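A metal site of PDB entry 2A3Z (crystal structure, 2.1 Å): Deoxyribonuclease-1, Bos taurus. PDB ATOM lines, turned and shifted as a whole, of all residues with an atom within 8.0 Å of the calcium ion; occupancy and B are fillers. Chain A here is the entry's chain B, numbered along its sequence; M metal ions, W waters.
The side-chain hydroxyl (OG1) of Thr 205 sits at hydrogen-bond distance from the side-chain hydroxyl (OG1) of Thr 207 (3.1 Å).
The side-chain sulfur of Cys 209 sits close to the side-chain hydroxyl of Thr 207 (3.8 Å).
Of the 16 residues printed, 4 come within 4 Å of the calcium ion.
The nearest printed residue that does not touch the calcium ion is Ser 206 (4.4 Å).
The calcium ion is bound by the backbone carbonyl oxygen (O) of Thr 205 (2.4 Å), water W2 (2.4 Å), the backbone carbonyl oxygen (O) of Thr 207 (2.4 Å), water W1 (2.5 Å), the side-chain carboxylate (OD2) of Asp 201 (2.5 Å), the backbone carbonyl oxygen (O) of Thr 203 (2.5 Å), the side-chain hydroxyl (OG1) of Thr 203 (2.6 Å) and the side-chain carboxylate (OD1) of Asp 201 (2.6 Å).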
ATOM      1  N   ALA A 200      11.177  -2.196  15.358  1.00  0.00           N
ATOM      2  CA  ALA A 200      11.656  -0.813  15.144  1.00  0.00           C
ATOM      3  C   ALA A 200      13.173  -0.777  15.237  1.00  0.00           C
ATOM      4  O   ALA A 200      13.759  -1.496  16.045  1.00  0.00           O
ATOM      5  CB  ALA A 200      11.078   0.180  16.186  1.00  0.00           C
ATOM      6  N   ASP A 201      13.772   0.121  14.467  1.00  0.00           N
ATOM      7  CA  ASP A 201      15.201   0.238  14.513  1.00  0.00           C
ATOM      8  C   ASP A 201      15.458   1.539  15.243  1.00  0.00           C
ATOM      9  O   ASP A 201      15.082   2.613  14.758  1.00  0.00           O
ATOM     10  CB  ASP A 201      15.788   0.322  13.126  1.00  0.00           C
ATOM     11  CG  ASP A 201      17.283   0.641  13.129  1.00  0.00           C
ATOM     12  OD1 ASP A 201      17.955   0.338  14.143  1.00  0.00           O
ATOM     13  OD2 ASP A 201      17.834   1.087  12.098  1.00  0.00           O
ATOM     14  N   THR A 202      16.085   1.458  16.414  1.00  0.00           N
ATOM     15  CA  THR A 202      16.289   2.728  17.097  1.00  0.00           C
ATOM     16  C   THR A 202      17.754   3.099  17.232  1.00  0.00           C
ATOM     17  O   THR A 202      18.071   3.905  18.067  1.00  0.00           O
ATOM     18  CB  THR A 202      15.639   2.775  18.516  1.00  0.00           C
ATOM     19  OG1 THR A 202      16.457   2.005  19.423  1.00  0.00           O
ATOM     20  CG2 THR A 202      14.201   2.249  18.514  1.00  0.00           C
ATOM     21  N   THR A 203      18.651   2.463  16.468  1.00  0.00           N
ATOM     22  CA  THR A 203      20.048   2.786  16.551  1.00  0.00           C
ATOM     23  C   THR A 203      20.453   3.527  15.312  1.00  0.00           C
ATOM     24  O   THR A 203      19.957   3.214  14.220  1.00  0.00           O
ATOM     25  CB  THR A 203      20.917   1.534  16.679  1.00  0.00           C
ATOM     26  OG1 THR A 203      20.827   0.746  15.476  1.00  0.00           O
ATOM     27  CG2 THR A 203      20.518   0.666  17.920  1.00  0.00           C
ATOM     28  N   ALA A 204      21.357   4.496  15.461  1.00  0.00           N
ATOM     29  CA  ALA A 204      21.851   5.268  14.293  1.00  0.00           C
ATOM     30  C   ALA A 204      22.966   4.450  13.621  1.00  0.00           C
ATOM     31  O   ALA A 204      23.334   4.710  12.456  1.00  0.00           O
ATOM     32  CB  ALA A 204      22.338   6.679  14.691  1.00  0.00           C
ATOM     33  N   THR A 205      23.434   3.418  14.335  1.00  0.00           N
ATOM     34  CA  THR A 205      24.405   2.452  13.784  1.00  0.00           C
ATOM     35  C   THR A 205      23.773   1.434  12.841  1.00  0.00           C
ATOM     36  O   THR A 205      22.541   1.298  12.746  1.00  0.00           O
ATOM     37  CB  THR A 205      25.094   1.673  14.904  1.00  0.00           C
ATOM     38  OG1 THR A 205      24.140   0.801  15.529  1.00  0.00           O
ATOM     39  CG2 THR A 205      25.611   2.625  16.001  1.00  0.00           C
ATOM     40  N   SER A 206      24.615   0.673  12.169  1.00  0.00           N
ATOM     41  CA  SER A 206      24.150  -0.360  11.283  1.00  0.00           C
ATOM     42  C   SER A 206      23.546  -1.597  11.979  1.00  0.00           C
ATOM     43  O   SER A 206      23.229  -2.567  11.292  1.00  0.00           O
ATOM     44  CB  SER A 206      25.322  -0.796  10.410  1.00  0.00           C
ATOM     45  OG  SER A 206      26.119  -1.598  11.236  1.00  0.00           O
ATOM     46  N   THR A 207      23.384  -1.623  13.299  1.00  0.00           N
ATOM     47  CA  THR A 207      22.572  -2.720  13.877  1.00  0.00           C
ATOM     48  C   THR A 207      21.068  -2.432  13.659  1.00  0.00           C
ATOM     49  O   THR A 207      20.679  -1.274  13.517  1.00  0.00           O
ATOM     50  CB  THR A 207      22.785  -2.874  15.410  1.00  0.00           C
ATOM     51  OG1 THR A 207      22.357  -1.681  16.087  1.00  0.00           O
ATOM     52  CG2 THR A 207      24.270  -3.154  15.756  1.00  0.00           C
ATOM     53  N   ASN A 208      20.215  -3.464  13.672  1.00  0.00           N
ATOM     54  CA  ASN A 208      18.763  -3.249  13.540  1.00  0.00           C
ATOM     55  C   ASN A 208      18.223  -3.709  14.866  1.00  0.00           C
ATOM     56  O   ASN A 208      18.065  -4.932  15.040  1.00  0.00           O
ATOM     57  CB  ASN A 208      18.163  -4.100  12.429  1.00  0.00           C
ATOM     58  CG  ASN A 208      16.632  -4.091  12.471  1.00  0.00           C
ATOM     59  OD1 ASN A 208      16.032  -3.066  12.783  1.00  0.00           O
ATOM     60  ND2 ASN A 208      16.008  -5.213  12.164  1.00  0.00           N
ATOM     61  N   CYS A 209      18.009  -2.763  15.803  1.00  0.00           N
ATOM     62  CA  CYS A 209      17.619  -3.138  17.161  1.00  0.00           C
ATOM     63  C   CYS A 209      16.636  -2.121  17.743  1.00  0.00           C
ATOM     64  O   CYS A 209      16.831  -0.921  17.627  1.00  0.00           O
ATOM     65  CB  CYS A 209      18.827  -3.201  18.087  1.00  0.00           C
ATOM     66  SG  CYS A 209      20.138  -4.360  17.537  1.00  0.00           S
ATOM     67  N   ASP A 234      14.447   9.299  12.923  1.00  0.00           N
ATOM     68  CA  ASP A 234      15.711   9.036  12.219  1.00  0.00           C
ATOM     69  C   ASP A 234      16.256  10.392  11.746  1.00  0.00           C
ATOM     70  O   ASP A 234      15.891  10.878  10.650  1.00  0.00           O
ATOM     71  CB  ASP A 234      15.457   8.046  11.089  1.00  0.00           C
ATOM     72  CG  ASP A 234      16.661   7.835  10.172  1.00  0.00           C
ATOM     73  OD1 ASP A 234      17.683   8.536  10.282  1.00  0.00           O
ATOM     74  OD2 ASP A 234      16.554   6.982   9.281  1.00  0.00           O
ATOM     75  N   ASN A 243      26.149   9.212   7.248  1.00  0.00           N
ATOM     76  CA  ASN A 243      26.132   8.333   8.420  1.00  0.00           C
ATOM     77  C   ASN A 243      27.184   8.800   9.430  1.00  0.00           C
ATOM     78  O   ASN A 243      26.964   8.697  10.634  1.00  0.00           O
ATOM     79  CB  ASN A 243      26.312   6.863   8.062  1.00  0.00           C
ATOM     80  CG  ASN A 243      26.220   5.937   9.291  1.00  0.00           C
ATOM     81  OD1 ASN A 243      27.232   5.358   9.722  1.00  0.00           O
ATOM     82  ND2 ASN A 243      25.016   5.819   9.892  1.00  0.00           N
ATOM     83  N   LEU A 247      26.421   9.623  13.381  1.00  0.00           N
ATOM     84  CA  LEU A 247      27.057   8.925  14.478  1.00  0.00           C
ATOM     85  C   LEU A 247      27.797   9.881  15.413  1.00  0.00           C
ATOM     86  O   LEU A 247      27.981   9.592  16.613  1.00  0.00           O
ATOM     87  CB  LEU A 247      28.014   7.913  13.872  1.00  0.00           C
ATOM     88  CG  LEU A 247      27.682   6.410  13.846  1.00  0.00           C
ATOM     89  CD1 LEU A 247      26.238   6.102  13.844  1.00  0.00           C
ATOM     90  CD2 LEU A 247      28.467   5.630  12.782  1.00  0.00           C
ATOM     91  N   ASP A 251      24.744   7.323  18.850  1.00  0.00           N
ATOM     92  CA  ASP A 251      24.467   6.066  18.174  1.00  0.00           C
ATOM     93  C   ASP A 251      23.026   5.517  18.301  1.00  0.00           C
ATOM     94  O   ASP A 251      22.719   4.432  17.808  1.00  0.00           O
ATOM     95  CB  ASP A 251      25.546   5.069  18.524  1.00  0.00           C
ATOM     96  CG  ASP A 251      25.708   4.883  20.033  1.00  0.00           C
ATOM     97  OD1 ASP A 251      25.035   5.546  20.869  1.00  0.00           O
ATOM     98  OD2 ASP A 251      26.572   4.047  20.361  1.00  0.00           O
ATOM     99  N   HIS A 252      22.143   6.310  18.897  1.00  0.00           N
ATOM    100  CA  HIS A 252      20.725   6.028  19.007  1.00  0.00           C
ATOM    101  C   HIS A 252      19.878   7.110  18.345  1.00  0.00           C
ATOM    102  O   HIS A 252      20.280   8.235  18.289  1.00  0.00           O
ATOM    103  CB  HIS A 252      20.276   5.944  20.469  1.00  0.00           C
ATOM    104  CG  HIS A 252      20.856   4.776  21.192  1.00  0.00           C
ATOM    105  ND1 HIS A 252      20.123   3.648  21.505  1.00  0.00           N
ATOM    106  CD2 HIS A 252      22.119   4.551  21.650  1.00  0.00           C
ATOM    107  CE1 HIS A 252      20.909   2.776  22.121  1.00  0.00           C
ATOM    108  NE2 HIS A 252      22.121   3.293  22.213  1.00  0.00           N
ATOM    109  N   TYR A 253      18.702   6.747  17.841  1.00  0.00           N
ATOM    110  CA  TYR A 253      17.717   7.737  17.527  1.00  0.00           C
ATOM    111  C   TYR A 253      16.854   8.014  18.748  1.00  0.00           C
ATOM    112  O   TYR A 253      16.657   7.076  19.581  1.00  0.00           O
ATOM    113  CB  TYR A 253      16.777   7.281  16.405  1.00  0.00           C
ATOM    114  CG  TYR A 253      17.467   6.829  15.134  1.00  0.00           C
ATOM    115  CD1 TYR A 253      18.483   7.581  14.555  1.00  0.00           C
ATOM    116  CD2 TYR A 253      17.071   5.640  14.508  1.00  0.00           C
ATOM    117  CE1 TYR A 253      19.104   7.190  13.397  1.00  0.00           C
ATOM    118  CE2 TYR A 253      17.685   5.217  13.335  1.00  0.00           C
ATOM    119  CZ  TYR A 253      18.698   6.000  12.785  1.00  0.00           C
ATOM    120  OH  TYR A 253      19.322   5.583  11.648  1.00  0.00           O
HETATM  121 CA    CA M   1      20.200   1.042  12.938  1.00  0.00          CA
HETATM  122  O   HOH W   1      20.310   2.854  11.234  1.00  0.00           O
HETATM  123  O   HOH W   2      20.245  -0.095  10.835  1.00  0.00           O
